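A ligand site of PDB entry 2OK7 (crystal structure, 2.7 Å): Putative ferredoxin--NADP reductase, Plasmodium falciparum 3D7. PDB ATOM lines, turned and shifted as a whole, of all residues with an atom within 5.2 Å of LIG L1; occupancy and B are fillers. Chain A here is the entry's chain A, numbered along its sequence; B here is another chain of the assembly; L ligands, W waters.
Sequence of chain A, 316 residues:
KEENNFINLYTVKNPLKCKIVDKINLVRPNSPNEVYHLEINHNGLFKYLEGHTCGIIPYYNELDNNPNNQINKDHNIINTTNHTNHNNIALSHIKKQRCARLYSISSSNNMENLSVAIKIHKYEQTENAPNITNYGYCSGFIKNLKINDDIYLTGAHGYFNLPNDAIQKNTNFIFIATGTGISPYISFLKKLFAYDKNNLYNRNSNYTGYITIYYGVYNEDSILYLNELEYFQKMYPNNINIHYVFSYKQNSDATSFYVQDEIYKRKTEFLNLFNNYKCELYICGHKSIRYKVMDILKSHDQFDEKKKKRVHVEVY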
ATOM      1  N   THR A  53       8.343 -21.155  16.363  1.00  0.00           N
ATOM      2  CA  THR A  53       7.148 -21.209  17.195  1.00  0.00           C
ATOM      3  C   THR A  53       6.479 -22.590  17.113  1.00  0.00           C
ATOM      4  O   THR A  53       6.687 -23.341  16.158  1.00  0.00           O
ATOM      5  CB  THR A  53       6.129 -20.094  16.841  1.00  0.00           C
ATOM      6  OG1 THR A  53       5.959 -20.040  15.419  1.00  0.00           O
ATOM      7  CG2 THR A  53       6.608 -18.737  17.323  1.00  0.00           C
ATOM      8  N   ARG A 101      -2.812 -21.458  18.768  1.00  0.00           N
ATOM      9  CA  ARG A 101      -2.190 -20.209  19.177  1.00  0.00           C
ATOM     10  C   ARG A 101      -0.692 -20.438  19.158  1.00  0.00           C
ATOM     11  O   ARG A 101      -0.217 -21.487  19.604  1.00  0.00           O
ATOM     12  CB  ARG A 101      -2.623 -19.796  20.584  1.00  0.00           C
ATOM     13  CG  ARG A 101      -4.119 -19.902  20.892  1.00  0.00           C
ATOM     14  CD  ARG A 101      -4.890 -18.680  20.461  1.00  0.00           C
ATOM     15  NE  ARG A 101      -6.298 -18.772  20.812  1.00  0.00           N
ATOM     16  CZ  ARG A 101      -7.293 -18.273  20.072  1.00  0.00           C
ATOM     17  NH1 ARG A 101      -7.051 -17.635  18.938  1.00  0.00           N
ATOM     18  NH2 ARG A 101      -8.535 -18.390  20.494  1.00  0.00           N
ATOM     19  N   LEU A 102       0.051 -19.471  18.635  1.00  0.00           N
ATOM     20  CA  LEU A 102       1.497 -19.625  18.496  1.00  0.00           C
ATOM     21  C   LEU A 102       2.242 -19.175  19.741  1.00  0.00           C
ATOM     22  O   LEU A 102       1.868 -18.190  20.389  1.00  0.00           O
ATOM     23  CB  LEU A 102       2.011 -18.896  17.247  1.00  0.00           C
ATOM     24  CG  LEU A 102       1.452 -19.344  15.880  1.00  0.00           C
ATOM     25  CD1 LEU A 102       2.156 -18.618  14.750  1.00  0.00           C
ATOM     26  CD2 LEU A 102       1.554 -20.855  15.676  1.00  0.00           C
ATOM     27  N   TYR A 103       3.276 -19.934  20.098  1.00  0.00           N
ATOM     28  CA  TYR A 103       4.146 -19.650  21.242  1.00  0.00           C
ATOM     29  C   TYR A 103       5.584 -19.995  20.869  1.00  0.00           C
ATOM     30  O   TYR A 103       5.854 -21.034  20.259  1.00  0.00           O
ATOM     31  CB  TYR A 103       3.693 -20.429  22.482  1.00  0.00           C
ATOM     32  CG  TYR A 103       2.283 -20.079  22.919  1.00  0.00           C
ATOM     33  CD1 TYR A 103       1.201 -20.882  22.547  1.00  0.00           C
ATOM     34  CD2 TYR A 103       2.026 -18.918  23.653  1.00  0.00           C
ATOM     35  CE1 TYR A 103      -0.092 -20.549  22.911  1.00  0.00           C
ATOM     36  CE2 TYR A 103       0.720 -18.571  24.033  1.00  0.00           C
ATOM     37  CZ  TYR A 103      -0.327 -19.394  23.643  1.00  0.00           C
ATOM     38  OH  TYR A 103      -1.611 -19.055  23.997  1.00  0.00           O
ATOM     39  N   SER A 104       6.509 -19.115  21.240  1.00  0.00           N
ATOM     40  CA  SER A 104       7.922 -19.275  20.909  1.00  0.00           C
ATOM     41  C   SER A 104       8.586 -20.318  21.795  1.00  0.00           C
ATOM     42  O   SER A 104       8.429 -20.268  23.008  1.00  0.00           O
ATOM     43  CB  SER A 104       8.648 -17.935  21.018  1.00  0.00           C
ATOM     44  OG  SER A 104       8.154 -17.025  20.052  1.00  0.00           O
ATOM     45  N   ALA A 117       6.907 -20.355  27.121  1.00  0.00           N
ATOM     46  CA  ALA A 117       6.509 -19.347  28.126  1.00  0.00           C
ATOM     47  C   ALA A 117       5.194 -18.659  27.723  1.00  0.00           C
ATOM     48  O   ALA A 117       5.113 -17.997  26.681  1.00  0.00           O
ATOM     49  CB  ALA A 117       7.605 -18.312  28.300  1.00  0.00           C
ATOM     50  N   ILE A 118       4.165 -18.840  28.549  1.00  0.00           N
ATOM     51  CA  ILE A 118       2.810 -18.388  28.216  1.00  0.00           C
ATOM     52  C   ILE A 118       2.260 -17.395  29.242  1.00  0.00           C
ATOM     53  O   ILE A 118       2.036 -17.749  30.406  1.00  0.00           O
ATOM     54  CB  ILE A 118       1.825 -19.592  28.066  1.00  0.00           C
ATOM     55  CG1 ILE A 118       2.358 -20.541  26.993  1.00  0.00           C
ATOM     56  CG2 ILE A 118       0.403 -19.104  27.715  1.00  0.00           C
ATOM     57  CD1 ILE A 118       1.572 -21.769  26.807  1.00  0.00           C
ATOM     58  N   LYS A 119       2.057 -16.161  28.785  1.00  0.00           N
ATOM     59  CA  LYS A 119       1.396 -15.130  29.574  1.00  0.00           C
ATOM     60  C   LYS A 119      -0.113 -15.401  29.636  1.00  0.00           C
ATOM     61  O   LYS A 119      -0.737 -15.656  28.610  1.00  0.00           O
ATOM     62  CB  LYS A 119       1.688 -13.747  28.962  1.00  0.00           C
ATOM     63  CG  LYS A 119       0.897 -12.585  29.545  1.00  0.00           C
ATOM     64  CD  LYS A 119       1.428 -11.245  29.069  1.00  0.00           C
ATOM     65  CE  LYS A 119       0.582 -10.109  29.603  1.00  0.00           C
ATOM     66  NZ  LYS A 119       1.310  -8.801  29.522  1.00  0.00           N
ATOM     67  N   HIS A 121      -3.708 -14.151  29.905  1.00  0.00           N
ATOM     68  CA  HIS A 121      -4.480 -12.946  29.584  1.00  0.00           C
ATOM     69  C   HIS A 121      -5.815 -12.939  30.315  1.00  0.00           C
ATOM     70  O   HIS A 121      -6.571 -13.911  30.277  1.00  0.00           O
ATOM     71  CB  HIS A 121      -4.738 -12.849  28.084  1.00  0.00           C
ATOM     72  CG  HIS A 121      -3.496 -12.828  27.250  1.00  0.00           C
ATOM     73  ND1 HIS A 121      -2.866 -11.657  26.884  1.00  0.00           N
ATOM     74  CD2 HIS A 121      -2.747 -13.828  26.733  1.00  0.00           C
ATOM     75  CE1 HIS A 121      -1.797 -11.932  26.157  1.00  0.00           C
ATOM     76  NE2 HIS A 121      -1.703 -13.252  26.049  1.00  0.00           N
ATOM     77  N   LYS A 122      -6.082 -11.825  30.992  1.00  0.00           N
ATOM     78  CA  LYS A 122      -7.340 -11.630  31.720  1.00  0.00           C
ATOM     79  C   LYS A 122      -8.110 -10.404  31.215  1.00  0.00           C
ATOM     80  O   LYS A 122      -7.564  -9.550  30.503  1.00  0.00           O
ATOM     81  CB  LYS A 122      -7.069 -11.463  33.212  1.00  0.00           C
ATOM     82  CG  LYS A 122      -6.299 -12.599  33.831  1.00  0.00           C
ATOM     83  CD  LYS A 122      -5.323 -12.096  34.865  1.00  0.00           C
ATOM     84  CE  LYS A 122      -4.127 -13.027  34.937  1.00  0.00           C
ATOM     85  NZ  LYS A 122      -3.503 -13.042  36.284  1.00  0.00           N
ATOM     86  N   TYR A 123      -9.381 -10.356  31.578  1.00  0.00           N
ATOM     87  CA  TYR A 123     -10.219  -9.157  31.489  1.00  0.00           C
ATOM     88  C   TYR A 123     -11.266  -9.287  32.597  1.00  0.00           C
ATOM     89  O   TYR A 123     -11.515 -10.391  33.079  1.00  0.00           O
ATOM     90  CB  TYR A 123     -10.825  -8.958  30.087  1.00  0.00           C
ATOM     91  CG  TYR A 123     -11.477 -10.170  29.428  1.00  0.00           C
ATOM     92  CD1 TYR A 123     -12.866 -10.297  29.387  1.00  0.00           C
ATOM     93  CD2 TYR A 123     -10.708 -11.143  28.782  1.00  0.00           C
ATOM     94  CE1 TYR A 123     -13.481 -11.384  28.758  1.00  0.00           C
ATOM     95  CE2 TYR A 123     -11.310 -12.253  28.166  1.00  0.00           C
ATOM     96  CZ  TYR A 123     -12.694 -12.357  28.154  1.00  0.00           C
ATOM     97  OH  TYR A 123     -13.291 -13.434  27.538  1.00  0.00           O
ATOM     98  N   GLY A 136      -8.549 -15.375  28.562  1.00  0.00           N
ATOM     99  CA  GLY A 136      -8.429 -15.682  27.137  1.00  0.00           C
ATOM    100  C   GLY A 136      -8.605 -17.171  26.866  1.00  0.00           C
ATOM    101  O   GLY A 136      -8.493 -17.982  27.793  1.00  0.00           O
ATOM    102  N   TYR A 137      -8.870 -17.517  25.619  1.00  0.00           N
ATOM    103  CA  TYR A 137      -9.184 -18.896  25.230  1.00  0.00           C
ATOM    104  C   TYR A 137      -8.105 -19.907  25.628  1.00  0.00           C
ATOM    105  O   TYR A 137      -8.406 -20.873  26.337  1.00  0.00           O
ATOM    106  CB  TYR A 137      -9.486 -19.007  23.746  1.00  0.00           C
ATOM    107  CG  TYR A 137      -9.931 -20.381  23.300  1.00  0.00           C
ATOM    108  CD1 TYR A 137     -11.068 -20.984  23.852  1.00  0.00           C
ATOM    109  CD2 TYR A 137      -9.234 -21.081  22.316  1.00  0.00           C
ATOM    110  CE1 TYR A 137     -11.484 -22.243  23.433  1.00  0.00           C
ATOM    111  CE2 TYR A 137      -9.649 -22.350  21.894  1.00  0.00           C
ATOM    112  CZ  TYR A 137     -10.771 -22.921  22.456  1.00  0.00           C
ATOM    113  OH  TYR A 137     -11.190 -24.168  22.062  1.00  0.00           O
ATOM    114  N   CYS A 138      -6.881 -19.684  25.167  1.00  0.00           N
ATOM    115  CA  CYS A 138      -5.777 -20.593  25.503  1.00  0.00           C
ATOM    116  C   CYS A 138      -5.287 -20.338  26.923  1.00  0.00           C
ATOM    117  O   CYS A 138      -4.871 -21.269  27.590  1.00  0.00           O
ATOM    118  CB  CYS A 138      -4.616 -20.439  24.516  1.00  0.00           C
ATOM    119  SG  CYS A 138      -3.303 -21.683  24.659  1.00  0.00           S
ATOM    120  N   SER A 139      -5.368 -19.080  27.347  1.00  0.00           N
ATOM    121  CA  SER A 139      -4.953 -18.623  28.669  1.00  0.00           C
ATOM    122  C   SER A 139      -5.646 -19.408  29.789  1.00  0.00           C
ATOM    123  O   SER A 139      -4.985 -19.886  30.716  1.00  0.00           O
ATOM    124  CB  SER A 139      -5.205 -17.117  28.833  1.00  0.00           C
ATOM    125  OG  SER A 139      -4.374 -16.348  27.967  1.00  0.00           O
ATOM    126  N   THR A 180       7.115 -11.570  26.617  1.00  0.00           N
ATOM    127  CA  THR A 180       7.362 -12.958  26.229  1.00  0.00           C
ATOM    128  C   THR A 180       8.306 -13.085  25.028  1.00  0.00           C
ATOM    129  O   THR A 180       8.744 -14.190  24.675  1.00  0.00           O
ATOM    130  CB  THR A 180       6.043 -13.712  25.987  1.00  0.00           C
ATOM    131  OG1 THR A 180       5.238 -12.994  25.029  1.00  0.00           O
ATOM    132  CG2 THR A 180       5.254 -13.892  27.292  1.00  0.00           C
ATOM    133  N   SER A 183      11.730 -15.125  24.805  1.00  0.00           N
ATOM    134  CA  SER A 183      11.711 -16.586  24.602  1.00  0.00           C
ATOM    135  C   SER A 183      12.534 -17.111  23.429  1.00  0.00           C
ATOM    136  O   SER A 183      13.337 -18.027  23.645  1.00  0.00           O
ATOM    137  CB  SER A 183      10.280 -17.151  24.563  1.00  0.00           C
ATOM    138  OG  SER A 183       9.710 -17.197  25.853  1.00  0.00           O
ATOM    139  N   GLU A 314       9.567 -10.335  14.250  1.00  0.00           N
ATOM    140  CA  GLU A 314       8.440 -11.183  14.645  1.00  0.00           C
ATOM    141  C   GLU A 314       7.640 -10.499  15.744  1.00  0.00           C
ATOM    142  O   GLU A 314       7.853 -10.745  16.931  1.00  0.00           O
ATOM    143  CB  GLU A 314       8.906 -12.574  15.083  1.00  0.00           C
ATOM    144  CG  GLU A 314       7.815 -13.636  14.930  1.00  0.00           C
ATOM    145  CD  GLU A 314       8.258 -15.009  15.364  1.00  0.00           C
ATOM    146  OE1 GLU A 314       8.848 -15.130  16.465  1.00  0.00           O
ATOM    147  OE2 GLU A 314       8.002 -15.984  14.613  1.00  0.00           O
ATOM    148  N   TYR A 316       3.854  -9.399  17.541  1.00  0.00           N
ATOM    149  CA  TYR A 316       2.490  -9.827  17.799  1.00  0.00           C
ATOM    150  C   TYR A 316       1.819  -8.949  18.843  1.00  0.00           C
ATOM    151  O   TYR A 316       2.460  -8.492  19.788  1.00  0.00           O
ATOM    152  CB  TYR A 316       2.436 -11.310  18.212  1.00  0.00           C
ATOM    153  CG  TYR A 316       3.342 -11.721  19.364  1.00  0.00           C
ATOM    154  CD1 TYR A 316       2.863 -11.766  20.673  1.00  0.00           C
ATOM    155  CD2 TYR A 316       4.676 -12.082  19.138  1.00  0.00           C
ATOM    156  CE1 TYR A 316       3.696 -12.151  21.741  1.00  0.00           C
ATOM    157  CE2 TYR A 316       5.517 -12.453  20.200  1.00  0.00           C
ATOM    158  CZ  TYR A 316       5.008 -12.497  21.489  1.00  0.00           C
ATOM    159  OH  TYR A 316       5.818 -12.867  22.531  1.00  0.00           O
ATOM    160  N   LEU B 102     -13.179 -11.161  17.629  1.00  0.00           N
ATOM    161  CA  LEU B 102     -14.106 -10.114  18.030  1.00  0.00           C
ATOM    162  C   LEU B 102     -13.762  -8.786  17.388  1.00  0.00           C
ATOM    163  O   LEU B 102     -12.586  -8.463  17.237  1.00  0.00           O
ATOM    164  CB  LEU B 102     -14.135  -9.983  19.552  1.00  0.00           C
ATOM    165  CG  LEU B 102     -14.355 -11.246  20.391  1.00  0.00           C
ATOM    166  CD1 LEU B 102     -14.238 -10.902  21.843  1.00  0.00           C
ATOM    167  CD2 LEU B 102     -15.689 -11.910  20.127  1.00  0.00           C
ATOM    168  N   GLU B 314     -12.100  -1.848  27.919  1.00  0.00           N
ATOM    169  CA  GLU B 314     -12.047  -2.969  26.951  1.00  0.00           C
ATOM    170  C   GLU B 314     -10.729  -2.876  26.170  1.00  0.00           C
ATOM    171  O   GLU B 314     -10.623  -2.135  25.191  1.00  0.00           O
ATOM    172  CB  GLU B 314     -13.272  -3.013  26.005  1.00  0.00           C
ATOM    173  CG  GLU B 314     -13.842  -4.414  25.786  1.00  0.00           C
ATOM    174  CD  GLU B 314     -15.018  -4.497  24.793  1.00  0.00           C
ATOM    175  OE1 GLU B 314     -15.011  -3.710  23.812  1.00  0.00           O
ATOM    176  OE2 GLU B 314     -15.916  -5.345  25.002  1.00  0.00           O
ATOM    177  N   VAL B 315      -9.738  -3.640  26.643  1.00  0.00           N
ATOM    178  CA  VAL B 315      -8.367  -3.592  26.088  1.00  0.00           C
ATOM    179  C   VAL B 315      -7.950  -4.842  25.297  1.00  0.00           C
ATOM    180  O   VAL B 315      -8.243  -5.970  25.699  1.00  0.00           O
ATOM    181  CB  VAL B 315      -7.297  -3.226  27.168  1.00  0.00           C
ATOM    182  CG1 VAL B 315      -7.464  -1.788  27.644  1.00  0.00           C
ATOM    183  CG2 VAL B 315      -7.295  -4.199  28.351  1.00  0.00           C
ATOM    184  N   TYR B 316      -7.263  -4.633  24.164  1.00  0.00           N
ATOM    185  CA  TYR B 316      -6.871  -5.733  23.266  1.00  0.00           C
ATOM    186  C   TYR B 316      -5.563  -5.530  22.501  1.00  0.00           C
ATOM    187  O   TYR B 316      -4.766  -4.667  22.849  1.00  0.00           O
ATOM    188  CB  TYR B 316      -8.010  -6.074  22.291  1.00  0.00           C
ATOM    189  CG  TYR B 316      -8.497  -4.940  21.399  1.00  0.00           C
ATOM    190  CD1 TYR B 316      -7.930  -4.721  20.136  1.00  0.00           C
ATOM    191  CD2 TYR B 316      -9.555  -4.120  21.792  1.00  0.00           C
ATOM    192  CE1 TYR B 316      -8.382  -3.678  19.307  1.00  0.00           C
ATOM    193  CE2 TYR B 316     -10.017  -3.078  20.963  1.00  0.00           C
ATOM    194  CZ  TYR B 316      -9.428  -2.874  19.725  1.00  0.00           C
ATOM    195  OH  TYR B 316      -9.885  -1.858  18.909  1.00  0.00           O
HETATM  196  P1  LIG L   1      -7.786 -14.931  23.095  1.00  0.00           P
HETATM  197  O1  LIG L   1      -7.672 -15.789  21.865  1.00  0.00           O
HETATM  198  O2  LIG L   1      -9.182 -14.951  23.650  1.00  0.00           O
HETATM  199  O3  LIG L   1      -7.132 -13.508  22.760  1.00  0.00           O
HETATM  200  C1  LIG L   1      -7.841 -12.297  22.681  1.00  0.00           C
HETATM  201  C2  LIG L   1      -7.287 -11.267  23.663  1.00  0.00           C
HETATM  202  O4  LIG L   1      -8.326 -10.366  23.924  1.00  0.00           O
HETATM  203  C3  LIG L   1      -6.867 -11.787  25.047  1.00  0.00           C
HETATM  204  O5  LIG L   1      -5.797 -10.983  25.473  1.00  0.00           O
HETATM  205  C4  LIG L   1      -8.046 -11.555  25.964  1.00  0.00           C
HETATM  206  O6  LIG L   1      -7.677 -10.997  27.215  1.00  0.00           O
HETATM  207  C5  LIG L   1      -8.910 -10.553  25.209  1.00  0.00           C
HETATM  208  N1  LIG L   1     -10.306 -11.015  25.077  1.00  0.00           N
HETATM  209  C6  LIG L   1     -10.760 -12.234  24.642  1.00  0.00           C
HETATM  210  N2  LIG L   1     -12.115 -12.232  24.685  1.00  0.00           N
HETATM  211  C7  LIG L   1     -12.523 -11.025  25.134  1.00  0.00           C
HETATM  212  C8  LIG L   1     -13.788 -10.493  25.373  1.00  0.00           C
HETATM  213  N3  LIG L   1     -14.864 -11.257  25.236  1.00  0.00           N
HETATM  214  N4  LIG L   1     -13.899  -9.196  25.853  1.00  0.00           N
HETATM  215  C9  LIG L   1     -12.763  -8.447  26.100  1.00  0.00           C
HETATM  216  N5  LIG L   1     -11.508  -8.981  25.860  1.00  0.00           N
HETATM  217  C10 LIG L   1     -11.392 -10.248  25.390  1.00  0.00           C
HETATM  218  N6  LIG L   1       2.156 -15.271  23.742  1.00  0.00           N
HETATM  219  C11 LIG L   1       2.856 -15.664  24.854  1.00  0.00           C
HETATM  220  O7  LIG L   1       2.353 -15.543  25.976  1.00  0.00           O
HETATM  221  N7  LIG L   1       4.128 -16.192  24.700  1.00  0.00           N
HETATM  222  C12 LIG L   1       4.699 -16.332  23.453  1.00  0.00           C
HETATM  223  O8  LIG L   1       5.837 -16.801  23.334  1.00  0.00           O
HETATM  224  C13 LIG L   1       3.990 -15.943  22.319  1.00  0.00           C
HETATM  225  N8  LIG L   1       4.550 -16.073  21.065  1.00  0.00           N
HETATM  226  C14 LIG L   1       3.853 -15.695  19.937  1.00  0.00           C
HETATM  227  C15 LIG L   1       4.436 -15.840  18.678  1.00  0.00           C
HETATM  228  C16 LIG L   1       3.750 -15.460  17.519  1.00  0.00           C
HETATM  229  C17 LIG L   1       4.526 -15.321  16.232  1.00  0.00           C
HETATM  230  C18 LIG L   1       2.458 -14.926  17.644  1.00  0.00           C
HETATM  231  C19 LIG L   1       1.587 -14.699  16.450  1.00  0.00           C
HETATM  232  C20 LIG L   1       1.879 -14.807  18.916  1.00  0.00           C
HETATM  233  C21 LIG L   1       2.573 -15.172  20.069  1.00  0.00           C
HETATM  234  N9  LIG L   1       2.002 -15.038  21.335  1.00  0.00           N
HETATM  235  C22 LIG L   1       2.699 -15.419  22.472  1.00  0.00           C
HETATM  236  C23 LIG L   1       0.560 -14.632  21.464  1.00  0.00           C
HETATM  237  C24 LIG L   1      -0.357 -15.827  21.736  1.00  0.00           C
HETATM  238  O9  LIG L   1      -0.876 -16.294  20.510  1.00  0.00           O
HETATM  239  C25 LIG L   1      -1.456 -15.382  22.733  1.00  0.00           C
HETATM  240  O10 LIG L   1      -1.692 -16.311  23.779  1.00  0.00           O
HETATM  241  C26 LIG L   1      -2.778 -15.106  22.054  1.00  0.00           C
HETATM  242  O11 LIG L   1      -2.669 -14.104  21.068  1.00  0.00           O
HETATM  243  C27 LIG L   1      -3.808 -14.770  23.128  1.00  0.00           C
HETATM  244  O12 LIG L   1      -4.770 -15.754  22.913  1.00  0.00           O
HETATM  245  P2  LIG L   1      -5.632 -16.449  24.048  1.00  0.00           P
HETATM  246  O13 LIG L   1      -6.183 -17.730  23.489  1.00  0.00           O
HETATM  247  O14 LIG L   1      -4.901 -16.654  25.349  1.00  0.00           O
HETATM  248  O15 LIG L   1      -6.811 -15.390  24.272  1.00  0.00           O
HETATM  249  P1  LG2 L   2      -3.933 -13.706  13.951  1.00  0.00           P
HETATM  250  O1  LG2 L   2      -4.948 -14.161  14.959  1.00  0.00           O
HETATM  251  O2  LG2 L   2      -3.785 -14.712  12.828  1.00  0.00           O
HETATM  252  O3  LG2 L   2      -2.528 -13.390  14.677  1.00  0.00           O
HETATM  253  C1  LG2 L   2      -2.405 -12.334  15.617  1.00  0.00           C
HETATM  254  C2  LG2 L   2      -1.210 -11.425  15.303  1.00  0.00           C
HETATM  255  O4  LG2 L   2      -0.012 -12.153  15.127  1.00  0.00           O
HETATM  256  C3  LG2 L   2      -1.415 -10.605  14.044  1.00  0.00           C
HETATM  257  O5  LG2 L   2      -1.004  -9.295  14.343  1.00  0.00           O
HETATM  258  C4  LG2 L   2      -0.507 -11.221  12.996  1.00  0.00           C
HETATM  259  O6  LG2 L   2       0.091 -10.245  12.176  1.00  0.00           O
HETATM  260  C5  LG2 L   2       0.550 -11.957  13.835  1.00  0.00           C
HETATM  261  N1  LG2 L   2       0.924 -13.296  13.311  1.00  0.00           N
HETATM  262  C6  LG2 L   2       0.067 -14.347  13.071  1.00  0.00           C
HETATM  263  N2  LG2 L   2       0.792 -15.396  12.623  1.00  0.00           N
HETATM  264  C7  LG2 L   2       2.102 -15.045  12.593  1.00  0.00           C
HETATM  265  C8  LG2 L   2       3.246 -15.728  12.223  1.00  0.00           C
HETATM  266  N3  LG2 L   2       3.176 -16.994  11.801  1.00  0.00           N
HETATM  267  N4  LG2 L   2       4.462 -15.105  12.287  1.00  0.00           N
HETATM  268  C9  LG2 L   2       4.553 -13.793  12.713  1.00  0.00           C
HETATM  269  N5  LG2 L   2       3.399 -13.109  13.074  1.00  0.00           N
HETATM  270  C10 LG2 L   2       2.191 -13.721  13.013  1.00  0.00           C
HETATM  271  N6  LG2 L   2      -9.547  -5.457  15.826  1.00  0.00           N
HETATM  272  C11 LG2 L   2      -9.921  -4.495  14.904  1.00  0.00           C
HETATM  273  O7  LG2 L   2      -9.274  -4.358  13.864  1.00  0.00           O
HETATM  274  N7  LG2 L   2     -11.013  -3.684  15.147  1.00  0.00           N
HETATM  275  C12 LG2 L   2     -11.734  -3.825  16.315  1.00  0.00           C
HETATM  276  O8  LG2 L   2     -12.690  -3.088  16.508  1.00  0.00           O
HETATM  277  C13 LG2 L   2     -11.360  -4.793  17.256  1.00  0.00           C
HETATM  278  N8  LG2 L   2     -12.093  -4.926  18.427  1.00  0.00           N
HETATM  279  C14 LG2 L   2     -11.741  -5.882  19.351  1.00  0.00           C
HETATM  280  C15 LG2 L   2     -12.488  -5.996  20.518  1.00  0.00           C
HETATM  281  C16 LG2 L   2     -12.146  -6.954  21.474  1.00  0.00           C
HETATM  282  C17 LG2 L   2     -12.888  -6.951  22.775  1.00  0.00           C
HETATM  283  C18 LG2 L   2     -11.038  -7.794  21.231  1.00  0.00           C
HETATM  284  C19 LG2 L   2     -10.664  -8.923  22.139  1.00  0.00           C
HETATM  285  C20 LG2 L   2     -10.292  -7.677  20.054  1.00  0.00           C
HETATM  286  C21 LG2 L   2     -10.633  -6.726  19.118  1.00  0.00           C
HETATM  287  N9  LG2 L   2      -9.898  -6.602  17.944  1.00  0.00           N
HETATM  288  C22 LG2 L   2     -10.254  -5.621  17.007  1.00  0.00           C
HETATM  289  C23 LG2 L   2      -8.774  -7.581  17.675  1.00  0.00           C
HETATM  290  C24 LG2 L   2      -9.106  -8.586  16.589  1.00  0.00           C
HETATM  291  O9  LG2 L   2      -9.630  -9.757  17.174  1.00  0.00           O
HETATM  292  C25 LG2 L   2      -7.859  -8.808  15.716  1.00  0.00           C
HETATM  293  O10 LG2 L   2      -8.094  -8.631  14.337  1.00  0.00           O
HETATM  294  C26 LG2 L   2      -7.291 -10.195  15.824  1.00  0.00           C
HETATM  295  O11 LG2 L   2      -6.811 -10.469  17.120  1.00  0.00           O
HETATM  296  C27 LG2 L   2      -6.201 -10.308  14.760  1.00  0.00           C
HETATM  297  O12 LG2 L   2      -6.699 -11.409  14.048  1.00  0.00           O
HETATM  298  P2  LG2 L   2      -5.922 -12.119  12.857  1.00  0.00           P
HETATM  299  O13 LG2 L   2      -6.617 -13.449  12.645  1.00  0.00           O
HETATM  300  O14 LG2 L   2      -5.976 -11.243  11.644  1.00  0.00           O
HETATM  301  O15 LG2 L   2      -4.411 -12.288  13.365  1.00  0.00           O
HETATM  302  O   HOH W   1      -0.215 -15.682  25.927  1.00  0.00           O
HETATM  303  O   HOH W   2       7.170 -18.603  24.904  1.00  0.00           O
HETATM  304  O   HOH W   3     -11.835 -15.076  23.323  1.00  0.00           O
HETATM  305  O   HOH W   4      -5.082 -13.406  20.260  1.00  0.00           O
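O13 of LIG L1 lies within hydrogen-bond range of N of Cys 138, 2.7 Å away.
The backbone NH (N) of Ser 139 is in hydrogen-bond range of an oxygen (O14) of LIG L1, 3.2 Å away.
O14 of LIG L1 lies within hydrogen-bond range of OG of Ser 139 (2.7 Å).
An oxygen (O10) of LIG L1 is in hydrogen-bond range of the side-chain hydroxyl (OH) of Tyr 103, at 2.8 Å.
N7 of LIG L1 is in hydrogen-bond range of O of Ala 117.
An oxygen (O13) of LIG L1 lies within salt-bridge range of the guanidinium group (NE) of Arg 101, 2.9 Å away.
The backbone NH (N) of Lys 119 lies within hydrogen-bond range of an oxygen (O7) of LIG L1 (2.9 Å).
The backbone carbonyl oxygen (O) of Leu 102 of chain A lies close to an oxygen (O9) of LIG L1 (3.3 Å).
An oxygen (O8) of LIG L1 is in hydrogen-bond range of the backbone NH (N) of Ser 104.
The backbone NH (N) of Tyr 137 sits at hydrogen-bond distance from an oxygen (O2) of LIG L1, 3.2 Å away.
The side-chain hydroxyl (OH) of Tyr 123 sits at hydrogen-bond distance from a nitrogen (N2) of LIG L1, 3.3 Å away.
A ring nitrogen (ND1) of His 121 lies within hydrogen-bond range of an oxygen (O5) of LIG L1 (3.3 Å).
A nitrogen (N7) of LIG L1 lies close to the side-chain hydroxyl (OG1) of Thr 180 (3.4 Å).
The backbone carbonyl oxygen (O) of Leu 102 of chain B sits close to an oxygen (O9) of LG2 L2 (3.2 Å).
CG2 of Thr 53 touches C15 of LIG L1, 3.9 Å away.
Ile 118 touches LIG L1 (CA to O7, 3.6 Å).
O of Lys 122 touches O6 of LIG L1 (3.6 Å).
Gly 136 touches LIG L1.
CD of Glu 314 of chain A touches C17 of LIG L1, at 3.8 Å.
CE1 of Tyr 316 of chain A touches N9 of LIG L1, at 3.4 Å.
Leu 102 of chain B touches LIG L1 (CD1 to N3, 3.5 Å).
Of the 23 residues printed, 19 come within 4 Å of LIG L1.
Water W1 lies within hydrogen-bond range of O7 of LIG L1 (2.6 Å), O of Lys 119 (2.7 Å) and NE2 of His 121 (2.9 Å).
SG of Cys 138 sits at hydrogen-bond distance from OH of Tyr 103, at 3.2 Å.
OG of Ser 139 sits at hydrogen-bond distance from N of His 121.
N of Gly 136 is in hydrogen-bond range of O of His 121.
The side-chain hydroxyl (OG1) of Thr 180 is in hydrogen-bond range of the side-chain hydroxyl (OH) of Tyr 316 of chain A (2.6 Å).
The backbone carbonyl oxygen (O) of Thr 180 lies close to the side-chain hydroxyl (OG) of Ser 183 (3.4 Å).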
